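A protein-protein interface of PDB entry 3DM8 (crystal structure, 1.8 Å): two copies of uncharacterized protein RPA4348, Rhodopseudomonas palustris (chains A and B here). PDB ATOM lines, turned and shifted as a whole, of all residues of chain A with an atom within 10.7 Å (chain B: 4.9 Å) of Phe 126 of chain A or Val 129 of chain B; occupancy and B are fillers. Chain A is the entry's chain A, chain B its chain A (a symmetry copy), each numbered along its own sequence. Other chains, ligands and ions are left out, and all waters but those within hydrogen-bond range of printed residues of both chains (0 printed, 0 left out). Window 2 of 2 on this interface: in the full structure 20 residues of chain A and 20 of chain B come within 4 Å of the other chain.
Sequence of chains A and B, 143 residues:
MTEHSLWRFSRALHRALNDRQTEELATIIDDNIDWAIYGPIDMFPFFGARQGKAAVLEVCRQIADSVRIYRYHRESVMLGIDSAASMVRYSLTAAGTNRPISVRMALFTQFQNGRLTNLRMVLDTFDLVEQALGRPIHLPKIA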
ATOM      1  N   TYR A  38      32.741  -0.064 -15.566  1.00  0.00           N
ATOM      2  CA  TYR A  38      33.395  -1.359 -15.744  1.00  0.00           C
ATOM      3  C   TYR A  38      32.368  -2.403 -16.139  1.00  0.00           C
ATOM      4  O   TYR A  38      31.560  -2.849 -15.346  1.00  0.00           O
ATOM      5  CB  TYR A  38      34.160  -1.789 -14.480  1.00  0.00           C
ATOM      6  CG  TYR A  38      35.273  -0.813 -14.170  1.00  0.00           C
ATOM      7  CD1 TYR A  38      35.136   0.112 -13.147  1.00  0.00           C
ATOM      8  CD2 TYR A  38      36.426  -0.764 -14.940  1.00  0.00           C
ATOM      9  CE1 TYR A  38      36.094   1.018 -12.869  1.00  0.00           C
ATOM     10  CE2 TYR A  38      37.423   0.174 -14.652  1.00  0.00           C
ATOM     11  CZ  TYR A  38      37.224   1.070 -13.608  1.00  0.00           C
ATOM     12  OH  TYR A  38      38.154   2.024 -13.247  1.00  0.00           O
ATOM     13  N   GLY A  39      32.462  -2.846 -17.385  1.00  0.00           N
ATOM     14  CA  GLY A  39      31.594  -3.919 -17.838  1.00  0.00           C
ATOM     15  C   GLY A  39      31.957  -4.377 -19.235  1.00  0.00           C
ATOM     16  O   GLY A  39      32.874  -3.841 -19.844  1.00  0.00           O
ATOM     17  N   PRO A  40      31.254  -5.382 -19.735  1.00  0.00           N
ATOM     18  CA  PRO A  40      31.720  -6.101 -20.916  1.00  0.00           C
ATOM     19  C   PRO A  40      31.366  -5.387 -22.187  1.00  0.00           C
ATOM     20  O   PRO A  40      30.210  -5.388 -22.611  1.00  0.00           O
ATOM     21  CB  PRO A  40      30.977  -7.435 -20.848  1.00  0.00           C
ATOM     22  CG  PRO A  40      29.857  -7.254 -19.998  1.00  0.00           C
ATOM     23  CD  PRO A  40      30.126  -6.050 -19.081  1.00  0.00           C
ATOM     24  N   MET A  43      29.333  -6.850 -25.257  1.00  0.00           N
ATOM     25  CA  MET A  43      27.888  -6.797 -25.192  1.00  0.00           C
ATOM     26  C   MET A  43      27.362  -5.375 -25.166  1.00  0.00           C
ATOM     27  O   MET A  43      26.367  -5.059 -25.817  1.00  0.00           O
ATOM     28  CB  MET A  43      27.353  -7.491 -23.969  1.00  0.00           C
ATOM     29  CG  MET A  43      25.885  -7.688 -24.145  1.00  0.00           C
ATOM     30  SD  MET A  43      25.242  -8.916 -23.068  1.00  0.00           S
ATOM     31  CE  MET A  43      23.483  -8.544 -23.093  1.00  0.00           C
ATOM     32  N   PHE A  44      28.033  -4.536 -24.377  1.00  0.00           N
ATOM     33  CA  PHE A  44      27.616  -3.130 -24.173  1.00  0.00           C
ATOM     34  C   PHE A  44      28.726  -2.160 -24.588  1.00  0.00           C
ATOM     35  O   PHE A  44      29.586  -1.808 -23.781  1.00  0.00           O
ATOM     36  CB  PHE A  44      27.229  -2.888 -22.722  1.00  0.00           C
ATOM     37  CG  PHE A  44      26.267  -3.890 -22.171  1.00  0.00           C
ATOM     38  CD1 PHE A  44      26.706  -4.897 -21.325  1.00  0.00           C
ATOM     39  CD2 PHE A  44      24.937  -3.818 -22.472  1.00  0.00           C
ATOM     40  CE1 PHE A  44      25.798  -5.823 -20.801  1.00  0.00           C
ATOM     41  CE2 PHE A  44      24.034  -4.758 -21.970  1.00  0.00           C
ATOM     42  CZ  PHE A  44      24.458  -5.737 -21.138  1.00  0.00           C
ATOM     43  N   PHE A  47      30.168   0.764 -22.533  1.00  0.00           N
ATOM     44  CA  PHE A  47      31.000   0.591 -21.332  1.00  0.00           C
ATOM     45  C   PHE A  47      32.466   0.937 -21.608  1.00  0.00           C
ATOM     46  O   PHE A  47      32.903   1.176 -22.758  1.00  0.00           O
ATOM     47  CB  PHE A  47      30.837  -0.796 -20.716  1.00  0.00           C
ATOM     48  CG  PHE A  47      29.489  -1.019 -20.022  1.00  0.00           C
ATOM     49  CD1 PHE A  47      28.693   0.033 -19.649  1.00  0.00           C
ATOM     50  CD2 PHE A  47      29.050  -2.303 -19.758  1.00  0.00           C
ATOM     51  CE1 PHE A  47      27.465  -0.195 -19.035  1.00  0.00           C
ATOM     52  CE2 PHE A  47      27.833  -2.525 -19.122  1.00  0.00           C
ATOM     53  CZ  PHE A  47      27.070  -1.472 -18.749  1.00  0.00           C
ATOM     54  N   ILE A 101      14.930  -5.251 -17.127  1.00  0.00           N
ATOM     55  CA  ILE A 101      16.224  -5.492 -16.579  1.00  0.00           C
ATOM     56  C   ILE A 101      16.386  -4.643 -15.333  1.00  0.00           C
ATOM     57  O   ILE A 101      15.995  -3.511 -15.320  1.00  0.00           O
ATOM     58  CB  ILE A 101      17.332  -5.164 -17.598  1.00  0.00           C
ATOM     59  CG1 ILE A 101      17.221  -6.073 -18.835  1.00  0.00           C
ATOM     60  CG2 ILE A 101      18.731  -5.233 -16.896  1.00  0.00           C
ATOM     61  CD1 ILE A 101      18.132  -5.643 -19.967  1.00  0.00           C
ATOM     62  N   SER A 102      16.902  -5.258 -14.288  1.00  0.00           N
ATOM     63  CA  SER A 102      17.271  -4.526 -13.042  1.00  0.00           C
ATOM     64  C   SER A 102      18.781  -4.493 -12.945  1.00  0.00           C
ATOM     65  O   SER A 102      19.446  -5.516 -13.167  1.00  0.00           O
ATOM     66  CB  SER A 102      16.602  -5.216 -11.844  1.00  0.00           C
ATOM     67  OG  SER A 102      17.094  -4.769 -10.594  1.00  0.00           O
ATOM     68  N   VAL A 103      19.334  -3.322 -12.653  1.00  0.00           N
ATOM     69  CA  VAL A 103      20.786  -3.106 -12.610  1.00  0.00           C
ATOM     70  C   VAL A 103      21.172  -2.508 -11.275  1.00  0.00           C
ATOM     71  O   VAL A 103      20.647  -1.472 -10.905  1.00  0.00           O
ATOM     72  CB  VAL A 103      21.218  -2.141 -13.724  1.00  0.00           C
ATOM     73  CG1 VAL A 103      22.725  -2.013 -13.767  1.00  0.00           C
ATOM     74  CG2 VAL A 103      20.710  -2.641 -15.086  1.00  0.00           C
ATOM     75  N   ARG A 104      22.081  -3.173 -10.553  1.00  0.00           N
ATOM     76  CA  ARG A 104      22.573  -2.625  -9.318  1.00  0.00           C
ATOM     77  C   ARG A 104      23.987  -2.073  -9.528  1.00  0.00           C
ATOM     78  O   ARG A 104      24.869  -2.767 -10.045  1.00  0.00           O
ATOM     79  CB  ARG A 104      22.629  -3.687  -8.234  1.00  0.00           C
ATOM     80  CG  ARG A 104      23.072  -3.081  -6.982  1.00  0.00           C
ATOM     81  CD  ARG A 104      23.107  -4.060  -5.856  1.00  0.00           C
ATOM     82  NE  ARG A 104      21.857  -4.004  -5.082  1.00  0.00           N
ATOM     83  CZ  ARG A 104      20.919  -4.937  -5.105  1.00  0.00           C
ATOM     84  NH1 ARG A 104      20.994  -5.990  -5.910  1.00  0.00           N
ATOM     85  NH2 ARG A 104      19.849  -4.773  -4.359  1.00  0.00           N
ATOM     86  N   VAL A 122      30.932   0.608 -10.914  1.00  0.00           N
ATOM     87  CA  VAL A 122      30.959  -0.867 -10.843  1.00  0.00           C
ATOM     88  C   VAL A 122      29.539  -1.349 -10.750  1.00  0.00           C
ATOM     89  O   VAL A 122      28.760  -0.893  -9.924  1.00  0.00           O
ATOM     90  CB  VAL A 122      31.694  -1.352  -9.554  1.00  0.00           C
ATOM     91  CG1 VAL A 122      31.912  -2.880  -9.592  1.00  0.00           C
ATOM     92  CG2 VAL A 122      32.990  -0.650  -9.457  1.00  0.00           C
ATOM     93  N   LEU A 123      29.192  -2.329 -11.565  1.00  0.00           N
ATOM     94  CA  LEU A 123      27.909  -2.984 -11.406  1.00  0.00           C
ATOM     95  C   LEU A 123      27.944  -4.483 -11.527  1.00  0.00           C
ATOM     96  O   LEU A 123      28.982  -5.079 -11.812  1.00  0.00           O
ATOM     97  CB  LEU A 123      26.944  -2.470 -12.456  1.00  0.00           C
ATOM     98  CG  LEU A 123      27.381  -2.762 -13.868  1.00  0.00           C
ATOM     99  CD1 LEU A 123      26.165  -3.030 -14.660  1.00  0.00           C
ATOM    100  CD2 LEU A 123      28.157  -1.575 -14.418  1.00  0.00           C
ATOM    101  N   ASP A 124      26.826  -5.070 -11.132  1.00  0.00           N
ATOM    102  CA  ASP A 124      26.678  -6.559 -11.111  1.00  0.00           C
ATOM    103  C   ASP A 124      26.445  -6.988 -12.554  1.00  0.00           C
ATOM    104  O   ASP A 124      25.326  -7.146 -13.053  1.00  0.00           O
ATOM    105  CB  ASP A 124      25.604  -7.017 -10.088  1.00  0.00           C
ATOM    106  CG  ASP A 124      25.540  -8.557  -9.944  1.00  0.00           C
ATOM    107  OD1 ASP A 124      26.167  -9.274 -10.767  1.00  0.00           O
ATOM    108  OD2 ASP A 124      24.768  -9.064  -9.098  1.00  0.00           O
ATOM    109  N   THR A 125      27.581  -7.141 -13.214  1.00  0.00           N
ATOM    110  CA  THR A 125      27.666  -7.339 -14.645  1.00  0.00           C
ATOM    111  C   THR A 125      27.226  -8.751 -15.051  1.00  0.00           C
ATOM    112  O   THR A 125      26.664  -8.921 -16.103  1.00  0.00           O
ATOM    113  CB  THR A 125      29.067  -7.035 -15.193  1.00  0.00           C
ATOM    114  OG1 THR A 125      30.031  -7.646 -14.324  1.00  0.00           O
ATOM    115  CG2 THR A 125      29.269  -5.482 -15.296  1.00  0.00           C
ATOM    116  N   PHE A 126      27.453  -9.745 -14.203  1.00  0.00           N
ATOM    117  CA  PHE A 126      26.997 -11.089 -14.537  1.00  0.00           C
ATOM    118  C   PHE A 126      25.476 -11.131 -14.518  1.00  0.00           C
ATOM    119  O   PHE A 126      24.812 -11.662 -15.442  1.00  0.00           O
ATOM    120  CB  PHE A 126      27.638 -12.157 -13.619  1.00  0.00           C
ATOM    121  CG  PHE A 126      27.276 -13.582 -13.996  1.00  0.00           C
ATOM    122  CD1 PHE A 126      28.016 -14.254 -14.939  1.00  0.00           C
ATOM    123  CD2 PHE A 126      26.214 -14.222 -13.408  1.00  0.00           C
ATOM    124  CE1 PHE A 126      27.681 -15.535 -15.306  1.00  0.00           C
ATOM    125  CE2 PHE A 126      25.868 -15.510 -13.748  1.00  0.00           C
ATOM    126  CZ  PHE A 126      26.602 -16.173 -14.690  1.00  0.00           C
ATOM    127  N   ASP A 127      24.902 -10.560 -13.488  1.00  0.00           N
ATOM    128  CA  ASP A 127      23.445 -10.546 -13.353  1.00  0.00           C
ATOM    129  C   ASP A 127      22.851  -9.782 -14.520  1.00  0.00           C
ATOM    130  O   ASP A 127      21.846 -10.207 -15.126  1.00  0.00           O
ATOM    131  CB  ASP A 127      23.013  -9.920 -12.041  1.00  0.00           C
ATOM    132  CG  ASP A 127      21.562 -10.110 -11.774  1.00  0.00           C
ATOM    133  OD1 ASP A 127      20.900  -9.123 -11.465  1.00  0.00           O
ATOM    134  OD2 ASP A 127      21.084 -11.247 -11.863  1.00  0.00           O
ATOM    135  N   LEU A 128      23.537  -8.712 -14.917  1.00  0.00           N
ATOM    136  CA  LEU A 128      23.051  -7.871 -16.045  1.00  0.00           C
ATOM    137  C   LEU A 128      23.045  -8.703 -17.319  1.00  0.00           C
ATOM    138  O   LEU A 128      22.055  -8.744 -18.066  1.00  0.00           O
ATOM    139  CB  LEU A 128      23.912  -6.602 -16.262  1.00  0.00           C
ATOM    140  CG  LEU A 128      23.746  -5.737 -17.507  1.00  0.00           C
ATOM    141  CD1 LEU A 128      22.297  -5.274 -17.771  1.00  0.00           C
ATOM    142  CD2 LEU A 128      24.719  -4.494 -17.527  1.00  0.00           C
ATOM    143  N   VAL A 129      24.150  -9.393 -17.571  1.00  0.00           N
ATOM    144  CA  VAL A 129      24.313 -10.159 -18.836  1.00  0.00           C
ATOM    145  C   VAL A 129      23.282 -11.273 -18.850  1.00  0.00           C
ATOM    146  O   VAL A 129      22.667 -11.554 -19.874  1.00  0.00           O
ATOM    147  CB  VAL A 129      25.762 -10.741 -19.068  1.00  0.00           C
ATOM    148  CG1 VAL A 129      25.730 -11.867 -20.128  1.00  0.00           C
ATOM    149  CG2 VAL A 129      26.762  -9.643 -19.463  1.00  0.00           C
ATOM    150  N   GLU A 130      23.102 -11.927 -17.708  1.00  0.00           N
ATOM    151  CA  GLU A 130      22.138 -13.018 -17.634  1.00  0.00           C
ATOM    152  C   GLU A 130      20.736 -12.564 -17.954  1.00  0.00           C
ATOM    153  O   GLU A 130      19.968 -13.234 -18.700  1.00  0.00           O
ATOM    154  CB  GLU A 130      22.141 -13.698 -16.280  1.00  0.00           C
ATOM    155  CG  GLU A 130      23.361 -14.574 -16.093  1.00  0.00           C
ATOM    156  CD  GLU A 130      23.051 -15.939 -15.495  1.00  0.00           C
ATOM    157  OE1 GLU A 130      22.188 -16.028 -14.581  1.00  0.00           O
ATOM    158  OE2 GLU A 130      23.708 -16.926 -15.923  1.00  0.00           O
ATOM    159  N   GLN A 131      20.382 -11.425 -17.379  1.00  0.00           N
ATOM    160  CA  GLN A 131      19.035 -10.873 -17.594  1.00  0.00           C
ATOM    161  C   GLN A 131      18.830 -10.462 -19.035  1.00  0.00           C
ATOM    162  O   GLN A 131      17.746 -10.685 -19.615  1.00  0.00           O
ATOM    163  CB  GLN A 131      18.790  -9.663 -16.702  1.00  0.00           C
ATOM    164  CG  GLN A 131      18.576  -9.948 -15.262  1.00  0.00           C
ATOM    165  CD  GLN A 131      18.361  -8.642 -14.520  1.00  0.00           C
ATOM    166  OE1 GLN A 131      17.267  -8.055 -14.564  1.00  0.00           O
ATOM    167  NE2 GLN A 131      19.407  -8.160 -13.861  1.00  0.00           N
ATOM    168  N   ALA A 132      19.876  -9.906 -19.638  1.00  0.00           N
ATOM    169  CA  ALA A 132      19.789  -9.425 -21.034  1.00  0.00           C
ATOM    170  C   ALA A 132      19.653 -10.597 -22.027  1.00  0.00           C
ATOM    171  O   ALA A 132      18.930 -10.500 -23.043  1.00  0.00           O
ATOM    172  CB  ALA A 132      21.005  -8.531 -21.393  1.00  0.00           C
ATOM    173  N   LEU A 133      20.315 -11.720 -21.726  1.00  0.00           N
ATOM    174  CA  LEU A 133      20.378 -12.877 -22.657  1.00  0.00           C
ATOM    175  C   LEU A 133      19.166 -13.751 -22.403  1.00  0.00           C
ATOM    176  O   LEU A 133      18.643 -14.430 -23.309  1.00  0.00           O
ATOM    177  CB  LEU A 133      21.614 -13.759 -22.437  1.00  0.00           C
ATOM    178  CG  LEU A 133      23.038 -13.303 -22.782  1.00  0.00           C
ATOM    179  CD1 LEU A 133      24.072 -14.333 -22.298  1.00  0.00           C
ATOM    180  CD2 LEU A 133      23.214 -13.028 -24.235  1.00  0.00           C
ATOM    181  N   GLY A 134      18.752 -13.726 -21.146  1.00  0.00           N
ATOM    182  CA  GLY A 134      17.494 -14.303 -20.674  1.00  0.00           C
ATOM    183  C   GLY A 134      17.725 -15.774 -20.476  1.00  0.00           C
ATOM    184  O   GLY A 134      16.783 -16.572 -20.343  1.00  0.00           O
ATOM    185  N   ARG A 135      19.014 -16.104 -20.518  1.00  0.00           N
ATOM    186  CA  ARG A 135      19.532 -17.469 -20.350  1.00  0.00           C
ATOM    187  C   ARG A 135      20.895 -17.453 -19.648  1.00  0.00           C
ATOM    188  O   ARG A 135      21.505 -16.377 -19.492  1.00  0.00           O
ATOM    189  CB  ARG A 135      19.703 -18.149 -21.709  1.00  0.00           C
ATOM    190  CG  ARG A 135      18.417 -18.381 -22.447  1.00  0.00           C
ATOM    191  CD  ARG A 135      18.567 -19.535 -23.405  1.00  0.00           C
ATOM    192  NE  ARG A 135      18.764 -20.796 -22.685  1.00  0.00           N
ATOM    193  CZ  ARG A 135      17.810 -21.696 -22.489  1.00  0.00           C
ATOM    194  NH1 ARG A 135      18.068 -22.809 -21.819  1.00  0.00           N
ATOM    195  NH2 ARG A 135      16.597 -21.487 -22.974  1.00  0.00           N
ATOM    196  N   PRO B  40      27.174 -14.320  -8.198  1.00  0.00           N
ATOM    197  CA  PRO B  40      26.465 -15.530  -8.598  1.00  0.00           C
ATOM    198  C   PRO B  40      26.763 -16.686  -7.688  1.00  0.00           C
ATOM    199  O   PRO B  40      27.845 -17.270  -7.744  1.00  0.00           O
ATOM    200  CB  PRO B  40      27.003 -15.823  -9.999  1.00  0.00           C
ATOM    201  CG  PRO B  40      28.232 -15.132 -10.133  1.00  0.00           C
ATOM    202  CD  PRO B  40      28.260 -13.978  -9.119  1.00  0.00           C
ATOM    203  N   MET B  43      28.163 -20.243  -8.730  1.00  0.00           N
ATOM    204  CA  MET B  43      29.596 -20.386  -8.870  1.00  0.00           C
ATOM    205  C   MET B  43      30.328 -20.175  -7.558  1.00  0.00           C
ATOM    206  O   MET B  43      31.272 -20.897  -7.240  1.00  0.00           O
ATOM    207  CB  MET B  43      30.168 -19.406  -9.859  1.00  0.00           C
ATOM    208  CG  MET B  43      31.557 -19.833 -10.194  1.00  0.00           C
ATOM    209  SD  MET B  43      32.136 -19.111 -11.685  1.00  0.00           S
ATOM    210  CE  MET B  43      33.914 -19.329 -11.534  1.00  0.00           C
ATOM    211  N   PHE B  44      29.892 -19.153  -6.823  1.00  0.00           N
ATOM    212  CA  PHE B  44      30.536 -18.756  -5.550  1.00  0.00           C
ATOM    213  C   PHE B  44      29.541 -18.814  -4.387  1.00  0.00           C
ATOM    214  O   PHE B  44      28.849 -17.836  -4.105  1.00  0.00           O
ATOM    215  CB  PHE B  44      31.129 -17.360  -5.658  1.00  0.00           C
ATOM    216  CG  PHE B  44      31.992 -17.155  -6.861  1.00  0.00           C
ATOM    217  CD1 PHE B  44      31.514 -16.454  -7.958  1.00  0.00           C
ATOM    218  CD2 PHE B  44      33.271 -17.632  -6.893  1.00  0.00           C
ATOM    219  CE1 PHE B  44      32.330 -16.253  -9.077  1.00  0.00           C
ATOM    220  CE2 PHE B  44      34.077 -17.454  -8.019  1.00  0.00           C
ATOM    221  CZ  PHE B  44      33.617 -16.764  -9.088  1.00  0.00           C
ATOM    222  N   THR B 125      31.313  -8.862 -11.688  1.00  0.00           N
ATOM    223  CA  THR B 125      31.025 -10.276 -11.578  1.00  0.00           C
ATOM    224  C   THR B 125      31.195 -10.997 -12.920  1.00  0.00           C
ATOM    225  O   THR B 125      31.592 -12.135 -12.939  1.00  0.00           O
ATOM    226  CB  THR B 125      29.629 -10.542 -10.999  1.00  0.00           C
ATOM    227  OG1 THR B 125      28.698  -9.668 -11.652  1.00  0.00           O
ATOM    228  CG2 THR B 125      29.649 -10.324  -9.444  1.00  0.00           C
ATOM    229  N   PHE B 126      30.928 -10.324 -14.031  1.00  0.00           N
ATOM    230  CA  PHE B 126      31.134 -10.966 -15.323  1.00  0.00           C
ATOM    231  C   PHE B 126      32.622 -11.182 -15.554  1.00  0.00           C
ATOM    232  O   PHE B 126      33.081 -12.278 -15.963  1.00  0.00           O
ATOM    233  CB  PHE B 126      30.458 -10.177 -16.470  1.00  0.00           C
ATOM    234  CG  PHE B 126      30.553 -10.862 -17.822  1.00  0.00           C
ATOM    235  CD1 PHE B 126      29.612 -11.791 -18.191  1.00  0.00           C
ATOM    236  CD2 PHE B 126      31.573 -10.568 -18.693  1.00  0.00           C
ATOM    237  CE1 PHE B 126      29.704 -12.435 -19.401  1.00  0.00           C
ATOM    238  CE2 PHE B 126      31.677 -11.188 -19.917  1.00  0.00           C
ATOM    239  CZ  PHE B 126      30.743 -12.117 -20.279  1.00  0.00           C
ATOM    240  N   ASP B 127      33.397 -10.162 -15.281  1.00  0.00           N
ATOM    241  CA  ASP B 127      34.845 -10.246 -15.473  1.00  0.00           C
ATOM    242  C   ASP B 127      35.399 -11.327 -14.566  1.00  0.00           C
ATOM    243  O   ASP B 127      36.247 -12.145 -14.977  1.00  0.00           O
ATOM    244  CB  ASP B 127      35.523  -8.920 -15.186  1.00  0.00           C
ATOM    245  CG  ASP B 127      36.951  -8.914 -15.603  1.00  0.00           C
ATOM    246  OD1 ASP B 127      37.786  -8.529 -14.788  1.00  0.00           O
ATOM    247  OD2 ASP B 127      37.239  -9.282 -16.747  1.00  0.00           O
ATOM    248  N   LEU B 128      34.837 -11.411 -13.361  1.00  0.00           N
ATOM    249  CA  LEU B 128      35.301 -12.423 -12.374  1.00  0.00           C
ATOM    250  C   LEU B 128      35.028 -13.816 -12.922  1.00  0.00           C
ATOM    251  O   LEU B 128      35.901 -14.698 -12.930  1.00  0.00           O
ATOM    252  CB  LEU B 128      34.620 -12.271 -10.991  1.00  0.00           C
ATOM    253  CG  LEU B 128      34.760 -13.344  -9.917  1.00  0.00           C
ATOM    254  CD1 LEU B 128      36.218 -13.730  -9.590  1.00  0.00           C
ATOM    255  CD2 LEU B 128      33.989 -12.988  -8.586  1.00  0.00           C
ATOM    256  N   VAL B 129      33.810 -14.024 -13.405  1.00  0.00           N
ATOM    257  CA  VAL B 129      33.380 -15.370 -13.871  1.00  0.00           C
ATOM    258  C   VAL B 129      34.223 -15.744 -15.076  1.00  0.00           C
ATOM    259  O   VAL B 129      34.659 -16.882 -15.216  1.00  0.00           O
ATOM    260  CB  VAL B 129      31.843 -15.487 -14.211  1.00  0.00           C
ATOM    261  CG1 VAL B 129      31.576 -16.730 -15.092  1.00  0.00           C
ATOM    262  CG2 VAL B 129      30.977 -15.517 -12.942  1.00  0.00           C
ATOM    263  N   GLU B 130      34.442 -14.783 -15.967  1.00  0.00           N
ATOM    264  CA  GLU B 130      35.234 -15.058 -17.160  1.00  0.00           C
ATOM    265  C   GLU B 130      36.638 -15.494 -16.825  1.00  0.00           C
ATOM    266  O   GLU B 130      37.201 -16.458 -17.417  1.00  0.00           O
ATOM    267  CB  GLU B 130      35.296 -13.868 -18.096  1.00  0.00           C
ATOM    268  CG  GLU B 130      33.990 -13.667 -18.836  1.00  0.00           C
ATOM    269  CD  GLU B 130      34.163 -13.386 -20.322  1.00  0.00           C
ATOM    270  OE1 GLU B 130      35.109 -12.643 -20.700  1.00  0.00           O
ATOM    271  OE2 GLU B 130      33.319 -13.886 -21.112  1.00  0.00           O
ATOM    272  N   GLN B 131      37.226 -14.777 -15.880  1.00  0.00           N
ATOM    273  CA  GLN B 131      38.604 -15.085 -15.464  1.00  0.00           C
ATOM    274  C   GLN B 131      38.690 -16.439 -14.796  1.00  0.00           C
ATOM    275  O   GLN B 131      39.649 -17.205 -15.026  1.00  0.00           O
ATOM    276  CB  GLN B 131      39.134 -14.031 -14.501  1.00  0.00           C
ATOM    277  CG  GLN B 131      39.478 -12.717 -15.099  1.00  0.00           C
ATOM    278  CD  GLN B 131      39.975 -11.786 -14.008  1.00  0.00           C
ATOM    279  OE1 GLN B 131      41.130 -11.884 -13.563  1.00  0.00           O
ATOM    280  NE2 GLN B 131      39.102 -10.901 -13.547  1.00  0.00           N
ATOM    281  N   ALA B 132      37.673 -16.765 -14.004  1.00  0.00           N
ATOM    282  CA  ALA B 132      37.660 -18.045 -13.263  1.00  0.00           C
ATOM    283  C   ALA B 132      37.496 -19.247 -14.215  1.00  0.00           C
ATOM    284  O   ALA B 132      38.096 -20.324 -14.001  1.00  0.00           O
ATOM    285  CB  ALA B 132      36.556 -18.045 -12.173  1.00  0.00           C
ATOM    286  N   LEU B 133      36.716 -19.064 -15.286  1.00  0.00           N
ATOM    287  CA  LEU B 133      36.367 -20.173 -16.212  1.00  0.00           C
ATOM    288  C   LEU B 133      37.456 -20.270 -17.261  1.00  0.00           C
ATOM    289  O   LEU B 133      37.758 -21.353 -17.799  1.00  0.00           O
ATOM    290  CB  LEU B 133      35.049 -19.938 -16.962  1.00  0.00           C
ATOM    291  CG  LEU B 133      33.678 -19.976 -16.275  1.00  0.00           C
ATOM    292  CD1 LEU B 133      32.569 -19.542 -17.247  1.00  0.00           C
ATOM    293  CD2 LEU B 133      33.368 -21.309 -15.688  1.00  0.00           C
ATOM    294  N   GLY B 134      38.020 -19.106 -17.545  1.00  0.00           N
ATOM    295  CA  GLY B 134      39.226 -18.942 -18.355  1.00  0.00           C
ATOM    296  C   GLY B 134      38.804 -18.988 -19.795  1.00  0.00           C
ATOM    297  O   GLY B 134      39.625 -19.148 -20.713  1.00  0.00           O
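N of Asp 124 of chain A sits at hydrogen-bond distance from O of Arg 104 of chain A, 3.2 Å away. The side-chain carboxylate of Asp 124 of chain A lies within hydrogen-bond range of the backbone NH of Asp 127 of chain A, 3.3 Å away.
Among the printed residues, merely in contact across the chains: Pro 40 of chain A with Phe 126 of chain B (3.8 Å), Phe 126 of chain A with Pro 40 of chain B (3.8 Å), Phe 126 of chain A with Phe 126 of chain B (3.5 Å), Phe 126 of chain A with Val 129 of chain B (3.8 Å) and Val 129 of chain A with Phe 126 of chain B (3.8 Å).
Pro 40 of chain A touches Phe 126 of chain B, and with the chains exchanged Phe 126 of chain A touches Pro 40 of chain B. Thr 125 of chain A touches Phe 126 of chain B, and with the chains exchanged Phe 126 of chain A touches Thr 125 of chain B. Phe 126 of chain B touches its own counterpart, Phe 126 of chain A. Phe 126 of chain A touches Val 129 of chain B, and with the chains exchanged Val 129 of chain A touches Phe 126 of chain B.
The side-chain hydroxyl (OG1) of Thr 125 of chain B sits at hydrogen-bond distance from the side-chain carboxylate (OD1) of Asp 124 of chain A (2.7 Å). The side-chain hydroxyl of Thr 125 of chain B sits at hydrogen-bond distance from the backbone NH of Thr 125 of chain A (3.2 Å). The side-chain hydroxyl (OG1) of Thr 125 of chain A lies within hydrogen-bond range of the backbone NH (N) of Phe 126 of chain B. OG1 of Thr 125 of chain B sits at hydrogen-bond distance from N of Phe 126 of chain A (2.8 Å).
Of the printed residues of chain B, Phe 126 of chain A touches Pro 40 (3.8 Å), Thr 125 (2.8 Å), Phe 126 (3.5 Å) and Val 129 (3.8 Å). Val 129 of chain B touches one residue of chain A. Thr 125 of chain B touches three residues of chain A. No residue of chain A comes within 4 Å of Glu 130 of chain B. Ala 132 of chain B touches none of the printed residues of chain A. Of the printed residues of chain B, Pro 40 of chain A touches Phe 126 (3.8 Å). Of the printed residues of chain B, Val 129 of chain A touches Phe 126 (3.8 Å). Of the printed residues of chain A, Phe 126 of chain B touches Pro 40, Thr 125, Phe 126 and Val 129. Val 103 of chain A touches none of the printed residues of chain B. The nearest residue of chain A that does not touch Val 129 of chain B is Thr 125 of chain A (7.5 Å).
Of the 13 printed residues of chain B, 4 touch a printed residue of chain A. Of the 24 printed residues of chain A, 5 touch a printed residue of chain B. Hydrophobic or aromatic side chains of chain A that line the printed part of chain B: Pro 40, Phe 126 and Val 129. Among the printed residues, no Asp or Glu carboxylate lies within 4 Å of a Lys or Arg side-chain nitrogen of the other chain.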
